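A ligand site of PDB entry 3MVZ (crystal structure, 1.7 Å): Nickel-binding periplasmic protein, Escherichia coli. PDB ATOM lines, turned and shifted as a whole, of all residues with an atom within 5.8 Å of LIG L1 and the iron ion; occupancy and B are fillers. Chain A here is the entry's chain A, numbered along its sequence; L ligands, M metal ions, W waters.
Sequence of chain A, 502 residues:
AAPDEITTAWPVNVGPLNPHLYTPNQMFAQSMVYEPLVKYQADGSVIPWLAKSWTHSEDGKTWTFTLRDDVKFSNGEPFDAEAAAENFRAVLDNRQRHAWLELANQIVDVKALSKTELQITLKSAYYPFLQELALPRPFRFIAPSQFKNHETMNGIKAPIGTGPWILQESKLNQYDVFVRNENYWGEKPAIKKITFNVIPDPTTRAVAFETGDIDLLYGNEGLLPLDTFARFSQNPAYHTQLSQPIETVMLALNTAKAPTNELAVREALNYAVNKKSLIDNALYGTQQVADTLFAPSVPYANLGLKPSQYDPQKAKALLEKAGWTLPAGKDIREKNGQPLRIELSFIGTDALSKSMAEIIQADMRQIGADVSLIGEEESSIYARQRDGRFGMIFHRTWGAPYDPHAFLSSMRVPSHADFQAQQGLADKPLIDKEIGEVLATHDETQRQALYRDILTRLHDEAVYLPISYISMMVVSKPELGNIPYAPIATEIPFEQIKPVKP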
ATOM      1  N   TYR A  22      -2.468   1.282  10.989  1.00  0.00           N
ATOM      2  CA  TYR A  22      -2.193   0.852  12.327  1.00  0.00           C
ATOM      3  C   TYR A  22      -0.747   0.371  12.499  1.00  0.00           C
ATOM      4  O   TYR A  22       0.086   0.834  11.839  1.00  0.00           O
ATOM      5  CB  TYR A  22      -3.215  -0.204  12.752  1.00  0.00           C
ATOM      6  CG  TYR A  22      -4.628   0.344  12.636  1.00  0.00           C
ATOM      7  CD1 TYR A  22      -5.322   0.332  11.451  1.00  0.00           C
ATOM      8  CD2 TYR A  22      -5.190   0.974  13.668  1.00  0.00           C
ATOM      9  CE1 TYR A  22      -6.560   0.874  11.366  1.00  0.00           C
ATOM     10  CE2 TYR A  22      -6.397   1.536  13.582  1.00  0.00           C
ATOM     11  CZ  TYR A  22      -7.108   1.482  12.439  1.00  0.00           C
ATOM     12  OH  TYR A  22      -8.349   2.072  12.390  1.00  0.00           O
ATOM     13  N   THR A  23      -0.487  -0.569  13.409  1.00  0.00           N
ATOM     14  CA  THR A  23       0.892  -1.042  13.518  1.00  0.00           C
ATOM     15  C   THR A  23       1.531  -1.325  12.114  1.00  0.00           C
ATOM     16  O   THR A  23       0.868  -1.921  11.256  1.00  0.00           O
ATOM     17  CB  THR A  23       0.994  -2.245  14.490  1.00  0.00           C
ATOM     18  OG1 THR A  23       2.379  -2.523  14.749  1.00  0.00           O
ATOM     19  CG2 THR A  23       0.309  -3.495  13.895  1.00  0.00           C
ATOM     20  N   MET A  27       0.705   5.419  17.699  1.00  0.00           N
ATOM     21  CA  MET A  27      -0.403   6.371  17.838  1.00  0.00           C
ATOM     22  C   MET A  27       0.087   7.694  18.409  1.00  0.00           C
ATOM     23  O   MET A  27      -0.427   8.684  17.889  1.00  0.00           O
ATOM     24  CB  MET A  27      -1.497   5.795  18.734  1.00  0.00           C
ATOM     25  CG  MET A  27      -1.865   4.354  18.410  1.00  0.00           C
ATOM     26  SD  MET A  27      -3.254   3.756  19.395  1.00  0.00           S
ATOM     27  CE  MET A  27      -4.478   5.015  19.035  1.00  0.00           C
ATOM     28  N   ARG A  97     -11.130  -2.451   7.568  1.00  0.00           N
ATOM     29  CA  ARG A  97      -9.982  -2.426   8.508  1.00  0.00           C
ATOM     30  C   ARG A  97     -10.317  -1.643   9.778  1.00  0.00           C
ATOM     31  O   ARG A  97      -9.702  -1.869  10.836  1.00  0.00           O
ATOM     32  CB  ARG A  97      -8.759  -1.824   7.800  1.00  0.00           C
ATOM     33  CG  ARG A  97      -7.490  -1.797   8.660  1.00  0.00           C
ATOM     34  CD  ARG A  97      -7.107  -3.219   9.061  1.00  0.00           C
ATOM     35  NE  ARG A  97      -5.940  -3.286   9.932  1.00  0.00           N
ATOM     36  CZ  ARG A  97      -5.958  -3.065  11.247  1.00  0.00           C
ATOM     37  NH1 ARG A  97      -4.823  -3.194  11.948  1.00  0.00           N
ATOM     38  NH2 ARG A  97      -7.086  -2.751  11.874  1.00  0.00           N
ATOM     39  N   TRP A 100     -13.422  -2.098  14.142  1.00  0.00           N
ATOM     40  CA  TRP A 100     -13.358  -1.921  15.588  1.00  0.00           C
ATOM     41  C   TRP A 100     -13.935  -0.573  16.076  1.00  0.00           C
ATOM     42  O   TRP A 100     -14.377  -0.464  17.209  1.00  0.00           O
ATOM     43  CB  TRP A 100     -11.915  -2.010  16.075  1.00  0.00           C
ATOM     44  CG  TRP A 100     -11.076  -0.830  15.663  1.00  0.00           C
ATOM     45  CD1 TRP A 100     -10.359  -0.689  14.507  1.00  0.00           C
ATOM     46  CD2 TRP A 100     -10.874   0.367  16.417  1.00  0.00           C
ATOM     47  NE1 TRP A 100      -9.731   0.541  14.491  1.00  0.00           N
ATOM     48  CE2 TRP A 100     -10.018   1.203  15.663  1.00  0.00           C
ATOM     49  CE3 TRP A 100     -11.335   0.813  17.669  1.00  0.00           C
ATOM     50  CZ2 TRP A 100      -9.614   2.474  16.103  1.00  0.00           C
ATOM     51  CZ3 TRP A 100     -10.923   2.073  18.130  1.00  0.00           C
ATOM     52  CH2 TRP A 100     -10.074   2.902  17.331  1.00  0.00           C
ATOM     53  N   ARG A 137      -6.189   8.195  15.484  1.00  0.00           N
ATOM     54  CA  ARG A 137      -6.417   7.613  14.141  1.00  0.00           C
ATOM     55  C   ARG A 137      -7.783   6.924  14.146  1.00  0.00           C
ATOM     56  O   ARG A 137      -8.251   6.489  15.206  1.00  0.00           O
ATOM     57  CB  ARG A 137      -5.291   6.643  13.751  1.00  0.00           C
ATOM     58  CG  ARG A 137      -5.177   5.411  14.640  1.00  0.00           C
ATOM     59  CD  ARG A 137      -3.811   4.733  14.502  1.00  0.00           C
ATOM     60  NE  ARG A 137      -3.747   3.506  15.316  1.00  0.00           N
ATOM     61  CZ  ARG A 137      -2.631   2.798  15.536  1.00  0.00           C
ATOM     62  NH1 ARG A 137      -1.477   3.220  15.040  1.00  0.00           N
ATOM     63  NH2 ARG A 137      -2.676   1.665  16.258  1.00  0.00           N
ATOM     64  N   GLN A 385      -5.705 -14.231  21.036  1.00  0.00           N
ATOM     65  CA  GLN A 385      -6.750 -13.290  21.431  1.00  0.00           C
ATOM     66  C   GLN A 385      -7.850 -13.235  20.371  1.00  0.00           C
ATOM     67  O   GLN A 385      -9.029 -13.257  20.693  1.00  0.00           O
ATOM     68  CB  GLN A 385      -6.174 -11.888  21.613  1.00  0.00           C
ATOM     69  CG  GLN A 385      -5.419 -11.673  22.921  1.00  0.00           C
ATOM     70  CD  GLN A 385      -4.831 -10.280  23.031  1.00  0.00           C
ATOM     71  OE1 GLN A 385      -3.863 -10.085  23.762  1.00  0.00           O
ATOM     72  NE2 GLN A 385      -5.400  -9.315  22.315  1.00  0.00           N
ATOM     73  N   HIS A 395      -4.880  -8.742  29.395  1.00  0.00           N
ATOM     74  CA  HIS A 395      -5.583  -7.797  28.519  1.00  0.00           C
ATOM     75  C   HIS A 395      -5.567  -6.460  29.223  1.00  0.00           C
ATOM     76  O   HIS A 395      -5.157  -6.371  30.391  1.00  0.00           O
ATOM     77  CB  HIS A 395      -7.033  -8.307  28.304  1.00  0.00           C
ATOM     78  CG  HIS A 395      -7.757  -7.642  27.170  1.00  0.00           C
ATOM     79  ND1 HIS A 395      -7.120  -6.992  26.122  1.00  0.00           N
ATOM     80  CD2 HIS A 395      -9.084  -7.544  26.897  1.00  0.00           C
ATOM     81  CE1 HIS A 395      -8.018  -6.517  25.281  1.00  0.00           C
ATOM     82  NE2 HIS A 395      -9.221  -6.842  25.728  1.00  0.00           N
ATOM     83  N   ARG A 396      -6.002  -5.408  28.548  1.00  0.00           N
ATOM     84  CA  ARG A 396      -6.070  -4.110  29.195  1.00  0.00           C
ATOM     85  C   ARG A 396      -7.092  -3.276  28.485  1.00  0.00           C
ATOM     86  O   ARG A 396      -7.384  -3.519  27.308  1.00  0.00           O
ATOM     87  CB  ARG A 396      -4.705  -3.409  29.177  1.00  0.00           C
ATOM     88  CG  ARG A 396      -4.150  -3.016  27.790  1.00  0.00           C
ATOM     89  CD  ARG A 396      -2.650  -2.767  27.843  1.00  0.00           C
ATOM     90  NE  ARG A 396      -2.285  -1.665  28.736  1.00  0.00           N
ATOM     91  CZ  ARG A 396      -1.272  -1.681  29.606  1.00  0.00           C
ATOM     92  NH1 ARG A 396      -0.526  -2.774  29.783  1.00  0.00           N
ATOM     93  NH2 ARG A 396      -1.023  -0.595  30.348  1.00  0.00           N
ATOM     94  N   THR A 397      -7.618  -2.283  29.185  1.00  0.00           N
ATOM     95  CA  THR A 397      -8.494  -1.310  28.540  1.00  0.00           C
ATOM     96  C   THR A 397      -7.665  -0.209  27.879  1.00  0.00           C
ATOM     97  O   THR A 397      -6.421  -0.294  27.821  1.00  0.00           O
ATOM     98  CB  THR A 397      -9.568  -0.733  29.475  1.00  0.00           C
ATOM     99  OG1 THR A 397      -8.977   0.142  30.459  1.00  0.00           O
ATOM    100  CG2 THR A 397     -10.368  -1.870  30.156  1.00  0.00           C
ATOM    101  N   TRP A 398      -8.342   0.787  27.343  1.00  0.00           N
ATOM    102  CA  TRP A 398      -7.681   1.666  26.367  1.00  0.00           C
ATOM    103  C   TRP A 398      -7.433   3.088  26.834  1.00  0.00           C
ATOM    104  O   TRP A 398      -6.726   3.843  26.139  1.00  0.00           O
ATOM    105  CB  TRP A 398      -8.497   1.662  25.083  1.00  0.00           C
ATOM    106  CG  TRP A 398      -8.525   0.309  24.390  1.00  0.00           C
ATOM    107  CD1 TRP A 398      -7.706  -0.760  24.635  1.00  0.00           C
ATOM    108  CD2 TRP A 398      -9.391  -0.079  23.312  1.00  0.00           C
ATOM    109  NE1 TRP A 398      -8.026  -1.801  23.777  1.00  0.00           N
ATOM    110  CE2 TRP A 398      -9.054  -1.409  22.968  1.00  0.00           C
ATOM    111  CE3 TRP A 398     -10.435   0.558  22.615  1.00  0.00           C
ATOM    112  CZ2 TRP A 398      -9.719  -2.121  21.935  1.00  0.00           C
ATOM    113  CZ3 TRP A 398     -11.102  -0.157  21.596  1.00  0.00           C
ATOM    114  CH2 TRP A 398     -10.717  -1.472  21.252  1.00  0.00           C
ATOM    115  N   GLY A 399      -8.000   3.450  27.999  1.00  0.00           N
ATOM    116  CA  GLY A 399      -7.864   4.775  28.563  1.00  0.00           C
ATOM    117  C   GLY A 399      -8.767   5.788  27.870  1.00  0.00           C
ATOM    118  O   GLY A 399      -9.437   5.445  26.890  1.00  0.00           O
ATOM    119  N   TYR A 402     -11.386   6.354  25.012  1.00  0.00           N
ATOM    120  CA  TYR A 402     -11.938   5.071  24.584  1.00  0.00           C
ATOM    121  C   TYR A 402     -12.785   4.400  25.643  1.00  0.00           C
ATOM    122  O   TYR A 402     -13.707   3.637  25.316  1.00  0.00           O
ATOM    123  CB  TYR A 402     -10.828   4.093  24.219  1.00  0.00           C
ATOM    124  CG  TYR A 402      -9.910   4.526  23.119  1.00  0.00           C
ATOM    125  CD1 TYR A 402      -8.725   5.199  23.431  1.00  0.00           C
ATOM    126  CD2 TYR A 402     -10.182   4.233  21.792  1.00  0.00           C
ATOM    127  CE1 TYR A 402      -7.838   5.612  22.432  1.00  0.00           C
ATOM    128  CE2 TYR A 402      -9.289   4.641  20.765  1.00  0.00           C
ATOM    129  CZ  TYR A 402      -8.123   5.316  21.103  1.00  0.00           C
ATOM    130  OH  TYR A 402      -7.267   5.729  20.116  1.00  0.00           O
ATOM    131  N   HIS A 416     -11.645 -10.041  18.297  1.00  0.00           N
ATOM    132  CA  HIS A 416     -11.018  -9.352  19.437  1.00  0.00           C
ATOM    133  C   HIS A 416     -11.122 -10.256  20.660  1.00  0.00           C
ATOM    134  O   HIS A 416     -12.058 -11.063  20.778  1.00  0.00           O
ATOM    135  CB  HIS A 416     -11.749  -8.043  19.781  1.00  0.00           C
ATOM    136  CG  HIS A 416     -11.325  -6.842  18.964  1.00  0.00           C
ATOM    137  ND1 HIS A 416     -10.959  -6.930  17.646  1.00  0.00           N
ATOM    138  CD2 HIS A 416     -11.279  -5.526  19.295  1.00  0.00           C
ATOM    139  CE1 HIS A 416     -10.664  -5.714  17.191  1.00  0.00           C
ATOM    140  NE2 HIS A 416     -10.862  -4.847  18.172  1.00  0.00           N
ATOM    141  N   ALA A 417     -10.190 -10.094  21.598  1.00  0.00           N
ATOM    142  CA  ALA A 417     -10.178 -10.931  22.814  1.00  0.00           C
ATOM    143  C   ALA A 417     -11.472 -10.883  23.607  1.00  0.00           C
ATOM    144  O   ALA A 417     -11.902 -11.912  24.183  1.00  0.00           O
ATOM    145  CB  ALA A 417      -8.989 -10.556  23.722  1.00  0.00           C
ATOM    146  N   ASP A 418     -12.101  -9.720  23.661  1.00  0.00           N
ATOM    147  CA  ASP A 418     -13.287  -9.585  24.514  1.00  0.00           C
ATOM    148  C   ASP A 418     -14.473 -10.359  23.986  1.00  0.00           C
ATOM    149  O   ASP A 418     -15.145 -11.028  24.747  1.00  0.00           O
ATOM    150  CB  ASP A 418     -13.637  -8.134  24.767  1.00  0.00           C
ATOM    151  CG  ASP A 418     -12.487  -7.385  25.337  1.00  0.00           C
ATOM    152  OD1 ASP A 418     -12.345  -7.434  26.572  1.00  0.00           O
ATOM    153  OD2 ASP A 418     -11.709  -6.806  24.531  1.00  0.00           O
ATOM    154  N   THR A 490      -3.098   7.654  25.151  1.00  0.00           N
ATOM    155  CA  THR A 490      -2.103   7.162  24.190  1.00  0.00           C
ATOM    156  C   THR A 490      -1.238   8.254  23.604  1.00  0.00           C
ATOM    157  O   THR A 490      -0.297   7.983  22.864  1.00  0.00           O
ATOM    158  CB  THR A 490      -2.742   6.400  23.017  1.00  0.00           C
ATOM    159  OG1 THR A 490      -3.621   7.268  22.270  1.00  0.00           O
ATOM    160  CG2 THR A 490      -3.509   5.230  23.524  1.00  0.00           C
HETATM  161  C1  LIG L   1      -6.756  -3.825  19.235  1.00  0.00           C
HETATM  162  C2  LIG L   1      -7.615  -4.784  19.777  1.00  0.00           C
HETATM  163  C3  LIG L   1      -7.517  -5.161  21.118  1.00  0.00           C
HETATM  164  C4  LIG L   1      -6.560  -4.559  21.928  1.00  0.00           C
HETATM  165  C5  LIG L   1      -5.709  -3.582  21.402  1.00  0.00           C
HETATM  166  C6  LIG L   1      -5.820  -3.209  20.059  1.00  0.00           C
HETATM  167  O1  LIG L   1      -4.978  -2.289  19.545  1.00  0.00           O
HETATM  168  C7  LIG L   1      -6.948  -3.471  17.766  1.00  0.00           C
HETATM  169  N1  LIG L   1      -7.055  -2.004  17.578  1.00  0.00           N
HETATM  170  C8  LIG L   1      -8.249  -1.472  18.244  1.00  0.00           C
HETATM  171  C9  LIG L   1      -8.113   0.021  18.538  1.00  0.00           C
HETATM  172  N2  LIG L   1      -6.798   0.363  19.139  1.00  0.00           N
HETATM  173  C10 LIG L   1      -7.098   0.226  20.582  1.00  0.00           C
HETATM  174  C11 LIG L   1      -6.031   0.853  21.456  1.00  0.00           C
HETATM  175  C12 LIG L   1      -6.363   1.968  22.222  1.00  0.00           C
HETATM  176  C13 LIG L   1      -5.416   2.532  23.068  1.00  0.00           C
HETATM  177  C14 LIG L   1      -4.124   2.018  23.134  1.00  0.00           C
HETATM  178  C15 LIG L   1      -3.801   0.898  22.387  1.00  0.00           C
HETATM  179  C16 LIG L   1      -4.753   0.322  21.546  1.00  0.00           C
HETATM  180  O2  LIG L   1      -4.393  -0.746  20.804  1.00  0.00           O
HETATM  181  C17 LIG L   1      -7.147  -1.708  16.140  1.00  0.00           C
HETATM  182  C18 LIG L   1      -5.793  -2.023  15.543  1.00  0.00           C
HETATM  183  O3  LIG L   1      -4.812  -1.758  16.256  1.00  0.00           O
HETATM  184  C19 LIG L   1      -6.684   1.793  18.825  1.00  0.00           C
HETATM  185  O4  LIG L   1      -5.778  -2.549  14.414  1.00  0.00           O
HETATM  186  C20 LIG L   1      -5.977   1.900  17.491  1.00  0.00           C
HETATM  187  O5  LIG L   1      -5.367   0.895  17.107  1.00  0.00           O
HETATM  188  O6  LIG L   1      -6.079   2.959  16.851  1.00  0.00           O
HETATM  189  O1  LG2 L   2      -2.095  -0.358  19.652  1.00  0.00           O
HETATM  190  O2  LG2 L   2      -3.183  -0.205  18.687  1.00  0.00           O
HETATM  191 FE    FE M   1      -5.266  -0.844  18.274  1.00  0.00          FE
HETATM  192  O   HOH W   1      -3.933   3.124  26.393  1.00  0.00           O
HETATM  193  O   HOH W   2      -7.620   5.209  17.549  1.00  0.00           O
HETATM  194  O   HOH W   3      -2.326  -2.155  15.297  1.00  0.00           O
HETATM  195  O   HOH W   4      -4.162  -1.744  24.432  1.00  0.00           O
HETATM  196  O   HOH W   5      -6.043  -3.817  24.888  1.00  0.00           O
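NH1 of Arg 97 lies within salt-bridge range of O4 of LIG L1, at 2.7 Å. The guanidinium group (NE) of Arg 137 lies within salt-bridge range of an oxygen (O6) of LIG L1, at 2.8 Å. NH2 of Arg 137 lies close to O2 of LG2 L2 (3.1 Å).
NE1 of Trp 100 sits at hydrogen-bond distance from OH of Tyr 22 (2.9 Å).
CD2 of Tyr 22 touches O5 of LIG L1, 3.4 Å away. CE of Met 27 touches O6 of LIG L1, 3.4 Å away. CE3 of Trp 100 touches C9 of LIG L1, 3.4 Å away. CG of Trp 398 touches C12 of LIG L1, at 3.5 Å. Tyr 402 touches LIG L1 (CE1 to C12, 3.9 Å). His 416 touches LIG L1. Thr 490 touches LIG L1 (CG2 to C14, 3.3 Å). Hydrophobic or aromatic side chains that line LIG L1: Tyr 22, Met 27, Trp 100, Trp 398, Tyr 402 and His 416. Within 4 Å of LIG L1: Tyr 22, Met 27, Arg 97, Trp 100, Arg 137, Trp 398, Tyr 402, His 416 and Thr 490. The nearest printed residue that does not touch LIG L1 is His 395 (4.1 Å).
No residue comes within 4 Å of the iron ion.
The iron ion is bound by O1 of LIG L1 (1.9 Å). O5 of LIG L1 binds the iron ion (2.1 Å). The iron ion is bound by a nitrogen (N2) of LIG L1 (2.1 Å). The iron ion is bound by O2 of LG2 L2, 2.2 Å away. A nitrogen (N1) of LIG L1 binds the iron ion (2.2 Å). The iron ion is bound by O3 of LIG L1 (2.3 Å). The iron ion has six donor atoms within binding distance. Slightly farther from the iron ion lies an oxygen (O2) of LIG L1 (2.7 Å).
Water W2 lies within hydrogen-bond range of the side-chain hydroxyl (OH) of Tyr 402 (2.6 Å), the backbone carbonyl oxygen (O) of Arg 137 (2.7 Å) and an oxygen (O6) of LIG L1 (2.8 Å). Water W5 lies within hydrogen-bond range of the backbone carbonyl oxygen (O) of Arg 396 and the indole nitrogen (NE1) of Trp 398.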
